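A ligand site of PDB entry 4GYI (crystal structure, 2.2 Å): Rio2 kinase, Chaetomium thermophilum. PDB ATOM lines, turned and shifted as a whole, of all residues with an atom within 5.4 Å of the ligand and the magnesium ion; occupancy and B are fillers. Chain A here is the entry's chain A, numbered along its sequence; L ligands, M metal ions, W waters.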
ATOM      1  N   GLY A 106      19.447 -28.062  32.171  1.00  0.00           N
ATOM      2  CA  GLY A 106      20.266 -28.944  31.350  1.00  0.00           C
ATOM      3  C   GLY A 106      20.456 -30.332  31.934  1.00  0.00           C
ATOM      4  O   GLY A 106      19.924 -30.657  33.003  1.00  0.00           O
ATOM      5  N   LYS A 107      21.218 -31.166  31.245  1.00  0.00           N
ATOM      6  CA  LYS A 107      21.383 -32.543  31.667  1.00  0.00           C
ATOM      7  C   LYS A 107      22.347 -32.616  32.830  1.00  0.00           C
ATOM      8  O   LYS A 107      22.195 -33.459  33.725  1.00  0.00           O
ATOM      9  CB  LYS A 107      21.863 -33.425  30.519  1.00  0.00           C
ATOM     10  CG  LYS A 107      20.925 -33.438  29.313  1.00  0.00           C
ATOM     11  CD  LYS A 107      19.487 -33.779  29.739  1.00  0.00           C
ATOM     12  CE  LYS A 107      18.531 -33.809  28.552  1.00  0.00           C
ATOM     13  NZ  LYS A 107      18.854 -34.898  27.581  1.00  0.00           N
ATOM     14  N   GLU A 108      23.330 -31.708  32.833  1.00  0.00           N
ATOM     15  CA  GLU A 108      24.318 -31.735  33.909  1.00  0.00           C
ATOM     16  C   GLU A 108      24.476 -30.407  34.646  1.00  0.00           C
ATOM     17  O   GLU A 108      25.229 -30.323  35.615  1.00  0.00           O
ATOM     18  CB  GLU A 108      25.665 -32.299  33.441  1.00  0.00           C
ATOM     19  CG  GLU A 108      26.154 -31.794  32.095  1.00  0.00           C
ATOM     20  CD  GLU A 108      26.290 -32.921  31.072  1.00  0.00           C
ATOM     21  OE1 GLU A 108      25.470 -33.857  31.114  1.00  0.00           O
ATOM     22  OE2 GLU A 108      27.218 -32.878  30.253  1.00  0.00           O
ATOM     23  N   SER A 109      23.725 -29.396  34.254  1.00  0.00           N
ATOM     24  CA  SER A 109      23.783 -28.123  34.967  1.00  0.00           C
ATOM     25  C   SER A 109      22.564 -27.271  34.687  1.00  0.00           C
ATOM     26  O   SER A 109      21.855 -27.497  33.716  1.00  0.00           O
ATOM     27  CB  SER A 109      25.044 -27.354  34.568  1.00  0.00           C
ATOM     28  OG  SER A 109      24.869 -26.743  33.296  1.00  0.00           O
ATOM     29  N   ASP A 110      22.300 -26.296  35.556  1.00  0.00           N
ATOM     30  CA  ASP A 110      21.264 -25.304  35.306  1.00  0.00           C
ATOM     31  C   ASP A 110      21.902 -23.942  35.000  1.00  0.00           C
ATOM     32  O   ASP A 110      22.837 -23.524  35.674  1.00  0.00           O
ATOM     33  CB  ASP A 110      20.321 -25.165  36.508  1.00  0.00           C
ATOM     34  CG  ASP A 110      19.410 -26.388  36.681  1.00  0.00           C
ATOM     35  OD1 ASP A 110      19.102 -27.053  35.667  1.00  0.00           O
ATOM     36  OD2 ASP A 110      19.015 -26.681  37.837  1.00  0.00           O
ATOM     37  N   ILE A 111      21.404 -23.260  33.981  1.00  0.00           N
ATOM     38  CA  ILE A 111      21.951 -21.974  33.597  1.00  0.00           C
ATOM     39  C   ILE A 111      20.902 -20.905  33.906  1.00  0.00           C
ATOM     40  O   ILE A 111      19.788 -20.974  33.421  1.00  0.00           O
ATOM     41  CB  ILE A 111      22.295 -21.931  32.092  1.00  0.00           C
ATOM     42  CG1 ILE A 111      23.197 -23.106  31.714  1.00  0.00           C
ATOM     43  CG2 ILE A 111      22.947 -20.609  31.723  1.00  0.00           C
ATOM     44  CD1 ILE A 111      24.589 -23.032  32.322  1.00  0.00           C
ATOM     45  N   VAL A 123      25.869 -14.655  33.984  1.00  0.00           N
ATOM     46  CA  VAL A 123      25.347 -16.012  34.033  1.00  0.00           C
ATOM     47  C   VAL A 123      25.690 -16.696  35.342  1.00  0.00           C
ATOM     48  O   VAL A 123      26.811 -16.598  35.832  1.00  0.00           O
ATOM     49  CB  VAL A 123      25.890 -16.868  32.854  1.00  0.00           C
ATOM     50  CG1 VAL A 123      25.753 -18.361  33.123  1.00  0.00           C
ATOM     51  CG2 VAL A 123      25.178 -16.492  31.567  1.00  0.00           C
ATOM     52  N   LYS A 125      25.898 -20.438  36.760  1.00  0.00           N
ATOM     53  CA  LYS A 125      25.840 -21.855  36.371  1.00  0.00           C
ATOM     54  C   LYS A 125      25.784 -22.685  37.649  1.00  0.00           C
ATOM     55  O   LYS A 125      26.561 -22.462  38.565  1.00  0.00           O
ATOM     56  CB  LYS A 125      27.058 -22.250  35.546  1.00  0.00           C
ATOM     57  CG  LYS A 125      27.059 -23.736  35.077  1.00  0.00           C
ATOM     58  CD  LYS A 125      28.259 -24.005  34.174  1.00  0.00           C
ATOM     59  CE  LYS A 125      28.363 -25.471  33.736  1.00  0.00           C
ATOM     60  NZ  LYS A 125      29.353 -25.629  32.617  1.00  0.00           N
ATOM     61  N   HIS A 127      25.932 -26.559  39.011  1.00  0.00           N
ATOM     62  CA  HIS A 127      26.254 -27.913  38.615  1.00  0.00           C
ATOM     63  C   HIS A 127      25.312 -28.930  39.247  1.00  0.00           C
ATOM     64  O   HIS A 127      24.971 -28.829  40.442  1.00  0.00           O
ATOM     65  CB  HIS A 127      27.708 -28.253  38.927  1.00  0.00           C
ATOM     66  CG  HIS A 127      28.694 -27.580  38.025  1.00  0.00           C
ATOM     67  ND1 HIS A 127      29.112 -28.137  36.831  1.00  0.00           N
ATOM     68  CD2 HIS A 127      29.353 -26.402  38.140  1.00  0.00           C
ATOM     69  CE1 HIS A 127      29.977 -27.334  36.252  1.00  0.00           C
ATOM     70  NE2 HIS A 127      30.145 -26.266  37.019  1.00  0.00           N
ATOM     71  N   GLU A 163      36.023 -26.049  37.225  1.00  0.00           N
ATOM     72  CA  GLU A 163      35.673 -25.245  36.055  1.00  0.00           C
ATOM     73  C   GLU A 163      36.105 -23.795  36.241  1.00  0.00           C
ATOM     74  O   GLU A 163      36.579 -23.136  35.300  1.00  0.00           O
ATOM     75  CB  GLU A 163      34.172 -25.345  35.711  1.00  0.00           C
ATOM     76  CG  GLU A 163      33.692 -24.340  34.632  1.00  0.00           C
ATOM     77  CD  GLU A 163      32.285 -24.646  34.082  1.00  0.00           C
ATOM     78  OE1 GLU A 163      31.372 -24.971  34.865  1.00  0.00           O
ATOM     79  OE2 GLU A 163      32.073 -24.555  32.849  1.00  0.00           O
ATOM     80  N   PRO A 178      34.426 -17.167  28.756  1.00  0.00           N
ATOM     81  CA  PRO A 178      33.743 -16.113  29.516  1.00  0.00           C
ATOM     82  C   PRO A 178      34.647 -15.596  30.622  1.00  0.00           C
ATOM     83  O   PRO A 178      35.512 -16.325  31.082  1.00  0.00           O
ATOM     84  CB  PRO A 178      32.543 -16.851  30.125  1.00  0.00           C
ATOM     85  CG  PRO A 178      32.348 -18.059  29.265  1.00  0.00           C
ATOM     86  CD  PRO A 178      33.728 -18.459  28.844  1.00  0.00           C
ATOM     87  N   MET A 190      29.503 -15.999  35.961  1.00  0.00           N
ATOM     88  CA  MET A 190      30.443 -15.622  34.928  1.00  0.00           C
ATOM     89  C   MET A 190      29.778 -14.613  33.986  1.00  0.00           C
ATOM     90  O   MET A 190      28.555 -14.454  34.011  1.00  0.00           O
ATOM     91  CB  MET A 190      30.853 -16.867  34.134  1.00  0.00           C
ATOM     92  CG  MET A 190      29.742 -17.385  33.238  1.00  0.00           C
ATOM     93  SD  MET A 190      30.112 -18.953  32.422  1.00  0.00           S
ATOM     94  CE  MET A 190      29.685 -20.123  33.694  1.00  0.00           C
ATOM     95  N   SER A 191      30.568 -13.933  33.158  1.00  0.00           N
ATOM     96  CA  SER A 191      30.009 -12.941  32.254  1.00  0.00           C
ATOM     97  C   SER A 191      29.059 -13.627  31.273  1.00  0.00           C
ATOM     98  O   SER A 191      29.166 -14.823  31.006  1.00  0.00           O
ATOM     99  CB  SER A 191      31.106 -12.199  31.482  1.00  0.00           C
ATOM    100  OG  SER A 191      31.710 -13.023  30.513  1.00  0.00           O
ATOM    101  N   LEU A 192      28.084 -12.864  30.805  1.00  0.00           N
ATOM    102  CA  LEU A 192      27.163 -13.332  29.777  1.00  0.00           C
ATOM    103  C   LEU A 192      27.786 -13.003  28.428  1.00  0.00           C
ATOM    104  O   LEU A 192      28.027 -11.843  28.135  1.00  0.00           O
ATOM    105  CB  LEU A 192      25.831 -12.599  29.917  1.00  0.00           C
ATOM    106  CG  LEU A 192      24.806 -12.752  28.795  1.00  0.00           C
ATOM    107  CD1 LEU A 192      24.326 -14.195  28.724  1.00  0.00           C
ATOM    108  CD2 LEU A 192      23.656 -11.796  29.052  1.00  0.00           C
ATOM    109  N   VAL A 193      28.075 -14.010  27.626  1.00  0.00           N
ATOM    110  CA  VAL A 193      28.729 -13.781  26.335  1.00  0.00           C
ATOM    111  C   VAL A 193      27.661 -13.482  25.298  1.00  0.00           C
ATOM    112  O   VAL A 193      26.666 -14.187  25.223  1.00  0.00           O
ATOM    113  CB  VAL A 193      29.516 -15.042  25.901  1.00  0.00           C
ATOM    114  CG1 VAL A 193      30.231 -14.804  24.594  1.00  0.00           C
ATOM    115  CG2 VAL A 193      30.521 -15.428  26.963  1.00  0.00           C
ATOM    116  N   ALA A 195      26.925 -14.364  22.375  1.00  0.00           N
ATOM    117  CA  ALA A 195      27.125 -15.342  21.333  1.00  0.00           C
ATOM    118  C   ALA A 195      26.184 -16.496  21.622  1.00  0.00           C
ATOM    119  O   ALA A 195      25.802 -16.727  22.767  1.00  0.00           O
ATOM    120  CB  ALA A 195      28.570 -15.827  21.305  1.00  0.00           C
ATOM    121  N   PRO A 197      25.207 -20.775  20.773  1.00  0.00           N
ATOM    122  CA  PRO A 197      25.855 -22.043  20.442  1.00  0.00           C
ATOM    123  C   PRO A 197      25.985 -22.226  18.924  1.00  0.00           C
ATOM    124  O   PRO A 197      25.064 -21.876  18.192  1.00  0.00           O
ATOM    125  CB  PRO A 197      24.890 -23.098  20.986  1.00  0.00           C
ATOM    126  CG  PRO A 197      24.126 -22.408  22.058  1.00  0.00           C
ATOM    127  CD  PRO A 197      24.048 -20.950  21.678  1.00  0.00           C
ATOM    128  N   ASP A 230      34.987 -32.076  25.825  1.00  0.00           N
ATOM    129  CA  ASP A 230      33.581 -32.042  25.395  1.00  0.00           C
ATOM    130  C   ASP A 230      33.418 -30.927  24.354  1.00  0.00           C
ATOM    131  O   ASP A 230      32.516 -30.096  24.429  1.00  0.00           O
ATOM    132  CB  ASP A 230      32.678 -31.841  26.621  1.00  0.00           C
ATOM    133  CG  ASP A 230      31.213 -32.082  26.306  1.00  0.00           C
ATOM    134  OD1 ASP A 230      30.949 -32.737  25.280  1.00  0.00           O
ATOM    135  OD2 ASP A 230      30.359 -31.604  27.090  1.00  0.00           O
ATOM    136  N   PHE A 234      27.753 -27.551  21.068  1.00  0.00           N
ATOM    137  CA  PHE A 234      27.028 -27.035  22.228  1.00  0.00           C
ATOM    138  C   PHE A 234      27.914 -26.225  23.158  1.00  0.00           C
ATOM    139  O   PHE A 234      27.423 -25.407  23.921  1.00  0.00           O
ATOM    140  CB  PHE A 234      26.385 -28.165  23.030  1.00  0.00           C
ATOM    141  CG  PHE A 234      25.434 -29.008  22.235  1.00  0.00           C
ATOM    142  CD1 PHE A 234      24.142 -28.583  22.025  1.00  0.00           C
ATOM    143  CD2 PHE A 234      25.857 -30.210  21.670  1.00  0.00           C
ATOM    144  CE1 PHE A 234      23.250 -29.355  21.278  1.00  0.00           C
ATOM    145  CE2 PHE A 234      24.981 -30.982  20.920  1.00  0.00           C
ATOM    146  CZ  PHE A 234      23.680 -30.552  20.719  1.00  0.00           C
ATOM    147  N   ASN A 235      29.229 -26.460  23.088  1.00  0.00           N
ATOM    148  CA  ASN A 235      30.165 -25.767  23.970  1.00  0.00           C
ATOM    149  C   ASN A 235      31.005 -24.746  23.248  1.00  0.00           C
ATOM    150  O   ASN A 235      31.980 -24.214  23.793  1.00  0.00           O
ATOM    151  CB  ASN A 235      31.047 -26.784  24.716  1.00  0.00           C
ATOM    152  CG  ASN A 235      30.228 -27.649  25.620  1.00  0.00           C
ATOM    153  OD1 ASN A 235      29.183 -27.203  26.090  1.00  0.00           O
ATOM    154  ND2 ASN A 235      30.640 -28.898  25.842  1.00  0.00           N
ATOM    155  N   LEU A 237      30.421 -21.218  21.297  1.00  0.00           N
ATOM    156  CA  LEU A 237      29.524 -20.124  21.038  1.00  0.00           C
ATOM    157  C   LEU A 237      30.143 -19.328  19.917  1.00  0.00           C
ATOM    158  O   LEU A 237      31.360 -19.231  19.825  1.00  0.00           O
ATOM    159  CB  LEU A 237      29.369 -19.241  22.304  1.00  0.00           C
ATOM    160  CG  LEU A 237      28.890 -19.919  23.605  1.00  0.00           C
ATOM    161  CD1 LEU A 237      28.438 -18.886  24.648  1.00  0.00           C
ATOM    162  CD2 LEU A 237      27.767 -20.897  23.363  1.00  0.00           C
ATOM    163  N   ILE A 257      33.170 -22.691  26.213  1.00  0.00           N
ATOM    164  CA  ILE A 257      32.669 -22.735  27.577  1.00  0.00           C
ATOM    165  C   ILE A 257      32.650 -24.198  28.020  1.00  0.00           C
ATOM    166  O   ILE A 257      32.893 -25.100  27.214  1.00  0.00           O
ATOM    167  CB  ILE A 257      31.225 -22.221  27.655  1.00  0.00           C
ATOM    168  CG1 ILE A 257      30.333 -23.125  26.808  1.00  0.00           C
ATOM    169  CG2 ILE A 257      31.095 -20.762  27.193  1.00  0.00           C
ATOM    170  CD1 ILE A 257      28.846 -22.845  26.908  1.00  0.00           C
ATOM    171  N   PHD A 258      32.325 -24.422  29.289  1.00  0.00           N
ATOM    172  CA  PHD A 258      32.005 -25.746  29.825  1.00  0.00           C
ATOM    173  C   PHD A 258      33.278 -26.528  30.067  1.00  0.00           C
ATOM    174  O   PHD A 258      33.699 -27.356  29.220  1.00  0.00           O
ATOM    175  CB  PHD A 258      30.959 -26.470  29.024  1.00  0.00           C
ATOM    176  CG  PHD A 258      30.376 -27.533  29.897  1.00  0.00           C
ATOM    177  OD1 PHD A 258      29.471 -28.405  29.383  1.00  0.00           O
ATOM    178  OD2 PHD A 258      30.804 -27.705  30.993  1.00  0.00           O
ATOM    179  P   PHD A 258      29.352 -29.775  30.224  1.00  0.00           P
ATOM    180  OP1 PHD A 258      29.291 -29.688  31.725  1.00  0.00           O
ATOM    181  OP2 PHD A 258      28.048 -30.490  29.865  1.00  0.00           O
ATOM    182  OP3 PHD A 258      30.576 -30.631  29.917  1.00  0.00           O
HETATM  183  P1  LIG L   1      26.282 -27.664  30.560  1.00  0.00           P
HETATM  184  O1  LIG L   1      24.992 -28.024  31.268  1.00  0.00           O
HETATM  185  O2  LIG L   1      26.472 -28.147  29.148  1.00  0.00           O
HETATM  186  O3  LIG L   1      27.467 -28.047  31.559  1.00  0.00           O
HETATM  187  P2  LIG L   1      27.293 -25.124  29.632  1.00  0.00           P
HETATM  188  O4  LIG L   1      27.703 -25.935  28.429  1.00  0.00           O
HETATM  189  O5  LIG L   1      28.394 -24.408  30.418  1.00  0.00           O
HETATM  190  O6  LIG L   1      26.419 -26.043  30.618  1.00  0.00           O
HETATM  191  O7  LIG L   1      26.165 -24.108  29.150  1.00  0.00           O
HETATM  192  C1  LIG L   1      24.972 -24.622  28.532  1.00  0.00           C
HETATM  193  C2  LIG L   1      24.402 -23.566  27.571  1.00  0.00           C
HETATM  194  O8  LIG L   1      24.181 -22.329  28.264  1.00  0.00           O
HETATM  195  C3  LIG L   1      25.329 -23.202  26.418  1.00  0.00           C
HETATM  196  O9  LIG L   1      25.203 -24.075  25.286  1.00  0.00           O
HETATM  197  C4  LIG L   1      24.921 -21.790  26.075  1.00  0.00           C
HETATM  198  O10 LIG L   1      23.682 -21.795  25.352  1.00  0.00           O
HETATM  199  C5  LIG L   1      24.551 -21.227  27.425  1.00  0.00           C
HETATM  200  N1  LIG L   1      25.663 -20.547  28.114  1.00  0.00           N
HETATM  201  C6  LIG L   1      26.412 -21.080  29.100  1.00  0.00           C
HETATM  202  N2  LIG L   1      27.328 -20.191  29.567  1.00  0.00           N
HETATM  203  C7  LIG L   1      27.134 -19.057  28.856  1.00  0.00           C
HETATM  204  C8  LIG L   1      27.740 -17.706  28.829  1.00  0.00           C
HETATM  205  N3  LIG L   1      28.746 -17.404  29.669  1.00  0.00           N
HETATM  206  N4  LIG L   1      27.247 -16.819  27.938  1.00  0.00           N
HETATM  207  C9  LIG L   1      26.229 -17.105  27.101  1.00  0.00           C
HETATM  208  N5  LIG L   1      25.629 -18.305  27.073  1.00  0.00           N
HETATM  209  C10 LIG L   1      26.040 -19.293  27.915  1.00  0.00           C
HETATM  210 MG    MG M   1      28.014 -27.819  27.743  1.00  0.00          MG
HETATM  211  O   HOH W   1      29.344 -21.855  30.919  1.00  0.00           O
HETATM  212  O   HOH W   2      22.257 -26.244  30.414  1.00  0.00           O
HETATM  213  O   HOH W   3      22.447 -25.209  24.266  1.00  0.00           O
HETATM  214  O   HOH W   4      22.023 -19.831  24.603  1.00  0.00           O
HETATM  215  O   HOH W   5      24.109 -17.983  24.569  1.00  0.00           O
HETATM  216  O   HOH W   6      26.454 -27.400  26.419  1.00  0.00           O
HETATM  217  O   HOH W   7      23.847 -30.412  30.525  1.00  0.00           O
HETATM  218  O   HOH W   8      27.763 -29.823  27.136  1.00  0.00           O
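The side-chain hydroxyl (OG) of Ser 109 lies within hydrogen-bond range of an oxygen (O1) of the ligand.
O of Phe 234 is in hydrogen-bond range of O9 of the ligand (2.9 Å).
A nitrogen (N3) of the ligand is in hydrogen-bond range of the backbone carbonyl oxygen (O) of Ser 191.
The side-chain sulfur of Met 190 is in hydrogen-bond range of a nitrogen (N3) of the ligand, 3.4 Å away.
N of Val 193 is in hydrogen-bond range of N4 of the ligand.
The side-chain amino group (NZ) of Lys 125 lies within salt-bridge range of an oxygen (O5) of the ligand, at 2.7 Å.
OD2 of Asp 230 lies close to OP3 of PHD 258 (3.0 Å).
OP2 of PHD 258 sits close to the side-chain carboxylate (OE2) of Glu 108, at 2.6 Å.
The backbone carbonyl oxygen (O) of Met 190 lies within hydrogen-bond range of the backbone NH (N) of Val 123.
The side-chain amide nitrogen (ND2) of Asn 235 sits at hydrogen-bond distance from the backbone carbonyl oxygen (O) of Asp 230.
OD2 of PHD 258 is in hydrogen-bond range of the side-chain amino group (NZ) of Lys 125 (3.0 Å).
The backbone carbonyl oxygen (O) of Asn 235 is in hydrogen-bond range of the backbone NH (N) of Ile 257, at 3.1 Å.
The side-chain amino group (NZ) of Lys 125 is in salt-bridge range of the side-chain carboxylate (OE2) of Glu 163 (2.9 Å).
CG1 of Ile 111 touches O8 of the ligand, 3.7 Å away.
Val 123 touches the ligand.
Pro 178 touches the ligand (CG to N3, 3.7 Å).
CD1 of Leu 192 touches C9 of the ligand (3.8 Å).
Pro 197 touches the ligand (CG to O10, 3.4 Å).
CD1 of Leu 237 touches C9 of the ligand, at 3.8 Å.
CD1 of Ile 257 touches C3 of the ligand, at 3.6 Å.
Hydrophobic or aromatic side chains that line the ligand: Ile 111, Val 123, Pro 178, Met 190, Leu 192, Val 193, Pro 197, Leu 237 and Ile 257.
The nearest printed residue that does not touch the ligand is Glu 108 (4.01 Å).
Of the 23 residues printed, 2 come within 4 Å of the magnesium ion.
The nearest printed residue that does not touch the magnesium ion is Asp 230 (4.5 Å).
The magnesium ion is bound by O4 of the ligand (2.0 Å), water W6 (2.1 Å), water W8 (2.1 Å), O2 of the ligand (2.1 Å), OD1 of Asn 235 (2.1 Å) and OD1 of PHD 258 (2.3 Å).
Water W8 lies within hydrogen-bond range of OP2 of PHD 258 (2.8 Å), OD2 of Asp 230 (3.1 Å) and ND2 of Asn 235 (3.3 Å).
Water W7 lies within hydrogen-bond range of the backbone NH of Glu 108 (2.7 Å), an oxygen (O1) of the ligand (2.8 Å) and the backbone NH of Lys 107 (2.8 Å).
Water W1 lies within hydrogen-bond range of O5 of the ligand (2.8 Å) and SD of Met 190 (3.4 Å).
Water W5 lies within hydrogen-bond range of the backbone carbonyl oxygen (O) of Ala 195 and a nitrogen (N5) of the ligand.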
